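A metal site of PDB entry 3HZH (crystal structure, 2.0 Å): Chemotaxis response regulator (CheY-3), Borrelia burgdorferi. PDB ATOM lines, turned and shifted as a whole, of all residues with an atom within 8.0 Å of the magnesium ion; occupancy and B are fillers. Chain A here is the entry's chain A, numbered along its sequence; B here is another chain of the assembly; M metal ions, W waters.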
ATOM      1  N   VAL A  42      36.135 -10.075  13.372  1.00  0.00           N
ATOM      2  CA  VAL A  42      35.898  -8.643  13.213  1.00  0.00           C
ATOM      3  C   VAL A  42      34.431  -8.294  12.907  1.00  0.00           C
ATOM      4  O   VAL A  42      33.929  -8.615  11.831  1.00  0.00           O
ATOM      5  CB  VAL A  42      36.775  -8.058  12.070  1.00  0.00           C
ATOM      6  CG1 VAL A  42      36.603  -6.543  12.001  1.00  0.00           C
ATOM      7  CG2 VAL A  42      38.234  -8.448  12.279  1.00  0.00           C
ATOM      8  N   ASP A  43      33.771  -7.637  13.853  1.00  0.00           N
ATOM      9  CA  ASP A  43      32.380  -7.226  13.682  1.00  0.00           C
ATOM     10  C   ASP A  43      32.097  -6.139  14.721  1.00  0.00           C
ATOM     11  O   ASP A  43      32.593  -6.214  15.841  1.00  0.00           O
ATOM     12  CB  ASP A  43      31.435  -8.415  13.875  1.00  0.00           C
ATOM     13  CG  ASP A  43      30.042  -8.139  13.353  1.00  0.00           C
ATOM     14  OD1 ASP A  43      29.325  -7.304  13.948  1.00  0.00           O
ATOM     15  OD2 ASP A  43      29.662  -8.760  12.336  1.00  0.00           O
ATOM     16  N   ASP A  44      31.316  -5.134  14.351  1.00  0.00           N
ATOM     17  CA  ASP A  44      31.016  -4.057  15.295  1.00  0.00           C
ATOM     18  C   ASP A  44      29.945  -4.400  16.342  1.00  0.00           C
ATOM     19  O   ASP A  44      29.604  -3.567  17.185  1.00  0.00           O
ATOM     20  CB  ASP A  44      30.642  -2.764  14.538  1.00  0.00           C
ATOM     21  CG  ASP A  44      29.454  -2.947  13.613  1.00  0.00           C
ATOM     22  OD1 ASP A  44      29.376  -3.997  12.974  1.00  0.00           O
ATOM     23  OD2 ASP A  44      28.629  -2.024  13.508  1.00  0.00           O
ATOM     24  N   SER A  45      29.425  -5.625  16.290  1.00  0.00           N
ATOM     25  CA  SER A  45      28.428  -6.058  17.266  1.00  0.00           C
ATOM     26  C   SER A  45      28.991  -7.111  18.218  1.00  0.00           C
ATOM     27  O   SER A  45      29.360  -8.197  17.793  1.00  0.00           O
ATOM     28  CB  SER A  45      27.195  -6.631  16.578  1.00  0.00           C
ATOM     29  OG  SER A  45      26.255  -7.081  17.550  1.00  0.00           O
ATOM     30  N   THR A  48      27.371 -10.480  17.777  1.00  0.00           N
ATOM     31  CA  THR A  48      27.895 -11.298  16.692  1.00  0.00           C
ATOM     32  C   THR A  48      29.283 -11.830  17.033  1.00  0.00           C
ATOM     33  O   THR A  48      29.613 -12.960  16.676  1.00  0.00           O
ATOM     34  CB  THR A  48      27.945 -10.480  15.393  1.00  0.00           C
ATOM     35  OG1 THR A  48      26.633  -9.960  15.126  1.00  0.00           O
ATOM     36  CG2 THR A  48      28.375 -11.355  14.232  1.00  0.00           C
ATOM     37  N   ALA A  68      36.339  -4.500  16.867  1.00  0.00           N
ATOM     38  CA  ALA A  68      35.008  -3.950  16.686  1.00  0.00           C
ATOM     39  C   ALA A  68      34.855  -3.010  15.484  1.00  0.00           C
ATOM     40  O   ALA A  68      33.757  -2.534  15.217  1.00  0.00           O
ATOM     41  CB  ALA A  68      34.556  -3.249  17.973  1.00  0.00           C
ATOM     42  N   BFD A  90      33.208  -8.527   9.030  1.00  0.00           N
ATOM     43  CA  BFD A  90      31.933  -7.886   8.808  1.00  0.00           C
ATOM     44  C   BFD A  90      32.189  -6.713   7.866  1.00  0.00           C
ATOM     45  O   BFD A  90      33.340  -6.292   7.676  1.00  0.00           O
ATOM     46  CB  BFD A  90      31.329  -7.409  10.142  1.00  0.00           C
ATOM     47  CG  BFD A  90      30.026  -6.620   9.960  1.00  0.00           C
ATOM     48  OD1 BFD A  90      29.178  -7.083   9.151  1.00  0.00           O
ATOM     49  OD2 BFD A  90      29.919  -5.569  10.628  1.00  0.00           O
ATOM     50 BE   BFD A  90      27.861  -6.411   8.716  1.00  0.00          BE
ATOM     51  F1  BFD A  90      27.536  -5.178   9.483  1.00  0.00           F
ATOM     52  F2  BFD A  90      28.025  -6.019   7.287  1.00  0.00           F
ATOM     53  F3  BFD A  90      26.710  -7.380   8.856  1.00  0.00           F
ATOM     54  N   ILE A  91      31.133  -6.168   7.271  1.00  0.00           N
ATOM     55  CA  ILE A  91      31.290  -5.045   6.361  1.00  0.00           C
ATOM     56  C   ILE A  91      30.871  -3.711   6.943  1.00  0.00           C
ATOM     57  O   ILE A  91      31.689  -2.797   7.041  1.00  0.00           O
ATOM     58  CB  ILE A  91      30.517  -5.287   5.039  1.00  0.00           C
ATOM     59  CG1 ILE A  91      31.193  -6.405   4.252  1.00  0.00           C
ATOM     60  CG2 ILE A  91      30.461  -3.995   4.208  1.00  0.00           C
ATOM     61  CD1 ILE A  91      30.482  -6.800   2.985  1.00  0.00           C
ATOM     62  N   THR A  92      29.617  -3.588   7.346  1.00  0.00           N
ATOM     63  CA  THR A  92      29.132  -2.334   7.892  1.00  0.00           C
ATOM     64  C   THR A  92      29.694  -2.107   9.284  1.00  0.00           C
ATOM     65  O   THR A  92      29.344  -2.797  10.222  1.00  0.00           O
ATOM     66  CB  THR A  92      27.581  -2.306   7.938  1.00  0.00           C
ATOM     67  OG1 THR A  92      27.090  -2.542   6.607  1.00  0.00           O
ATOM     68  CG2 THR A  92      27.071  -0.957   8.414  1.00  0.00           C
ATOM     69  N   MET A  93      30.571  -1.121   9.396  1.00  0.00           N
ATOM     70  CA  MET A  93      31.202  -0.842  10.675  1.00  0.00           C
ATOM     71  C   MET A  93      31.655   0.609  10.757  1.00  0.00           C
ATOM     72  O   MET A  93      31.972   1.223   9.752  1.00  0.00           O
ATOM     73  CB  MET A  93      32.449  -1.714  10.877  1.00  0.00           C
ATOM     74  CG  MET A  93      32.209  -3.221  11.024  1.00  0.00           C
ATOM     75  SD  MET A  93      33.755  -4.195  11.248  1.00  0.00           S
ATOM     76  CE  MET A  93      34.581  -3.979   9.643  1.00  0.00           C
ATOM     77  N   PRO A  94      31.678   1.177  11.974  1.00  0.00           N
ATOM     78  CA  PRO A  94      32.112   2.557  12.195  1.00  0.00           C
ATOM     79  C   PRO A  94      33.608   2.627  11.894  1.00  0.00           C
ATOM     80  O   PRO A  94      34.264   1.580  11.772  1.00  0.00           O
ATOM     81  CB  PRO A  94      31.854   2.767  13.683  1.00  0.00           C
ATOM     82  CG  PRO A  94      30.735   1.784  13.976  1.00  0.00           C
ATOM     83  CD  PRO A  94      31.283   0.576  13.258  1.00  0.00           C
ATOM     84  N   GLY A  98      34.299  -3.038   6.334  1.00  0.00           N
ATOM     85  CA  GLY A  98      35.003  -4.259   5.944  1.00  0.00           C
ATOM     86  C   GLY A  98      35.595  -4.341   4.542  1.00  0.00           C
ATOM     87  O   GLY A  98      36.528  -5.125   4.310  1.00  0.00           O
ATOM     88  N   ILE A 117      31.614 -11.959   6.358  1.00  0.00           N
ATOM     89  CA  ILE A 117      30.399 -12.414   7.016  1.00  0.00           C
ATOM     90  C   ILE A 117      29.596 -11.138   7.242  1.00  0.00           C
ATOM     91  O   ILE A 117      29.866 -10.363   8.166  1.00  0.00           O
ATOM     92  CB  ILE A 117      30.713 -13.104   8.376  1.00  0.00           C
ATOM     93  CG1 ILE A 117      31.629 -14.308   8.141  1.00  0.00           C
ATOM     94  CG2 ILE A 117      29.411 -13.542   9.062  1.00  0.00           C
ATOM     95  CD1 ILE A 117      31.896 -15.147   9.393  1.00  0.00           C
ATOM     96  N   SER A 118      28.599 -10.911   6.398  1.00  0.00           N
ATOM     97  CA  SER A 118      27.815  -9.678   6.476  1.00  0.00           C
ATOM     98  C   SER A 118      26.332  -9.781   6.159  1.00  0.00           C
ATOM     99  O   SER A 118      25.875 -10.737   5.541  1.00  0.00           O
ATOM    100  CB  SER A 118      28.447  -8.641   5.564  1.00  0.00           C
ATOM    101  OG  SER A 118      27.556  -7.566   5.271  1.00  0.00           O
ATOM    102  N   ALA A 119      25.584  -8.762   6.593  1.00  0.00           N
ATOM    103  CA  ALA A 119      24.136  -8.675   6.353  1.00  0.00           C
ATOM    104  C   ALA A 119      23.908  -8.262   4.901  1.00  0.00           C
ATOM    105  O   ALA A 119      22.796  -8.410   4.383  1.00  0.00           O
ATOM    106  CB  ALA A 119      23.523  -7.630   7.271  1.00  0.00           C
ATOM    107  N   LYS A 140      24.386 -13.162   6.540  1.00  0.00           N
ATOM    108  CA  LYS A 140      23.676 -13.329   7.810  1.00  0.00           C
ATOM    109  C   LYS A 140      22.164 -13.431   7.516  1.00  0.00           C
ATOM    110  O   LYS A 140      21.705 -12.983   6.459  1.00  0.00           O
ATOM    111  CB  LYS A 140      23.976 -12.132   8.718  1.00  0.00           C
ATOM    112  CG  LYS A 140      25.458 -11.896   8.988  1.00  0.00           C
ATOM    113  CD  LYS A 140      25.661 -10.632   9.833  1.00  0.00           C
ATOM    114  CE  LYS A 140      27.118 -10.439  10.258  1.00  0.00           C
ATOM    115  NZ  LYS A 140      27.276  -9.199  11.103  1.00  0.00           N
ATOM    116  N   THR B 106      20.540  -3.870  17.799  1.00  0.00           N
ATOM    117  CA  THR B 106      21.083  -3.109  16.673  1.00  0.00           C
ATOM    118  C   THR B 106      21.513  -4.071  15.561  1.00  0.00           C
ATOM    119  O   THR B 106      21.407  -3.742  14.387  1.00  0.00           O
ATOM    120  CB  THR B 106      22.300  -2.213  17.061  1.00  0.00           C
ATOM    121  OG1 THR B 106      23.332  -3.018  17.659  1.00  0.00           O
ATOM    122  CG2 THR B 106      21.872  -1.118  18.037  1.00  0.00           C
ATOM    123  N   GLU B 107      21.983  -5.262  15.939  1.00  0.00           N
ATOM    124  CA  GLU B 107      22.401  -6.233  14.933  1.00  0.00           C
ATOM    125  C   GLU B 107      21.177  -6.762  14.198  1.00  0.00           C
ATOM    126  O   GLU B 107      21.247  -7.080  13.009  1.00  0.00           O
ATOM    127  CB  GLU B 107      23.178  -7.403  15.560  1.00  0.00           C
ATOM    128  CG  GLU B 107      23.541  -8.503  14.571  1.00  0.00           C
ATOM    129  CD  GLU B 107      24.684  -8.128  13.639  1.00  0.00           C
ATOM    130  OE1 GLU B 107      24.810  -6.944  13.274  1.00  0.00           O
ATOM    131  OE2 GLU B 107      25.442  -9.043  13.225  1.00  0.00           O
ATOM    132  N   ASN B 110      20.494  -4.138  11.707  1.00  0.00           N
ATOM    133  CA  ASN B 110      21.507  -4.240  10.671  1.00  0.00           C
ATOM    134  C   ASN B 110      21.184  -5.360   9.680  1.00  0.00           C
ATOM    135  O   ASN B 110      21.349  -5.204   8.454  1.00  0.00           O
ATOM    136  CB  ASN B 110      22.875  -4.499  11.308  1.00  0.00           C
ATOM    137  CG  ASN B 110      23.952  -4.758  10.273  1.00  0.00           C
ATOM    138  OD1 ASN B 110      24.697  -5.738  10.388  1.00  0.00           O
ATOM    139  ND2 ASN B 110      24.055  -3.893   9.284  1.00  0.00           N
ATOM    140  N   ILE B 111      20.713  -6.489  10.190  1.00  0.00           N
ATOM    141  CA  ILE B 111      20.407  -7.620   9.319  1.00  0.00           C
ATOM    142  C   ILE B 111      19.147  -7.371   8.500  1.00  0.00           C
ATOM    143  O   ILE B 111      19.107  -7.711   7.314  1.00  0.00           O
ATOM    144  CB  ILE B 111      20.338  -8.925  10.137  1.00  0.00           C
ATOM    145  CG1 ILE B 111      21.692  -9.146  10.816  1.00  0.00           C
ATOM    146  CG2 ILE B 111      19.997 -10.120   9.233  1.00  0.00           C
ATOM    147  CD1 ILE B 111      21.732 -10.287  11.826  1.00  0.00           C
ATOM    148  N   ILE B 129      23.617   1.331   3.583  1.00  0.00           N
ATOM    149  CA  ILE B 129      23.091   1.487   4.938  1.00  0.00           C
ATOM    150  C   ILE B 129      24.216   1.990   5.836  1.00  0.00           C
ATOM    151  O   ILE B 129      25.386   1.899   5.486  1.00  0.00           O
ATOM    152  CB  ILE B 129      22.528   0.160   5.505  1.00  0.00           C
ATOM    153  CG1 ILE B 129      23.624  -0.884   5.644  1.00  0.00           C
ATOM    154  CG2 ILE B 129      21.424  -0.371   4.588  1.00  0.00           C
ATOM    155  CD1 ILE B 129      23.129  -2.203   6.255  1.00  0.00           C
ATOM    156  N   THR B 130      23.874   2.520   6.997  1.00  0.00           N
ATOM    157  CA  THR B 130      24.884   3.028   7.913  1.00  0.00           C
ATOM    158  C   THR B 130      25.019   2.123   9.127  1.00  0.00           C
ATOM    159  O   THR B 130      24.229   1.194   9.310  1.00  0.00           O
ATOM    160  CB  THR B 130      24.482   4.401   8.477  1.00  0.00           C
ATOM    161  OG1 THR B 130      23.447   4.220   9.451  1.00  0.00           O
ATOM    162  CG2 THR B 130      23.975   5.312   7.374  1.00  0.00           C
ATOM    163  N   PRO B 131      26.051   2.335   9.944  1.00  0.00           N
ATOM    164  CA  PRO B 131      26.213   1.521  11.140  1.00  0.00           C
ATOM    165  C   PRO B 131      24.974   1.878  11.964  1.00  0.00           C
ATOM    166  O   PRO B 131      24.436   2.981  11.833  1.00  0.00           O
ATOM    167  CB  PRO B 131      27.507   2.069  11.754  1.00  0.00           C
ATOM    168  CG  PRO B 131      28.294   2.449  10.494  1.00  0.00           C
ATOM    169  CD  PRO B 131      27.199   3.253   9.808  1.00  0.00           C
ATOM    170  N   PRO B 132      24.497   0.955  12.811  1.00  0.00           N
ATOM    171  CA  PRO B 132      23.293   1.252  13.590  1.00  0.00           C
ATOM    172  C   PRO B 132      23.461   2.121  14.832  1.00  0.00           C
ATOM    173  O   PRO B 132      24.556   2.262  15.376  1.00  0.00           O
ATOM    174  CB  PRO B 132      22.792  -0.142  13.939  1.00  0.00           C
ATOM    175  CG  PRO B 132      24.099  -0.822  14.285  1.00  0.00           C
ATOM    176  CD  PRO B 132      24.961  -0.413  13.085  1.00  0.00           C
HETATM  177 MG    MG M   1      28.201  -4.364  11.295  1.00  0.00          MG
HETATM  178  O   HOH W   1      26.766  -2.747  11.807  1.00  0.00           O
HETATM  179  O   HOH W   2      27.561  -6.386  12.214  1.00  0.00           O
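The magnesium ion is bound by the side-chain carboxylate of Asp 44 (2.1 Å), F1 of BFD 90 (2.1 Å), OD2 of BFD 90 (2.2 Å), the backbone carbonyl oxygen of Thr 92 (2.2 Å), water W1 (2.2 Å) and water W2 (2.3 Å).
OD1 of BFD 90 is in salt-bridge range of the side-chain amino group (NZ) of Lys 140 (3.5 Å). The backbone carbonyl oxygen (O) of Val 42 sits at hydrogen-bond distance from N of BFD 90 (2.9 Å). The side-chain amide oxygen (OD1) of Asn 110 of chain B lies close to the side-chain carboxylate (OE1) of Glu 107 of chain B (3.1 Å).
Asn 110 of chain B touches the magnesium ion. Within 4 Å of the magnesium ion: Asp 44, BFD 90, Thr 92 and Asn 110 of chain B.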
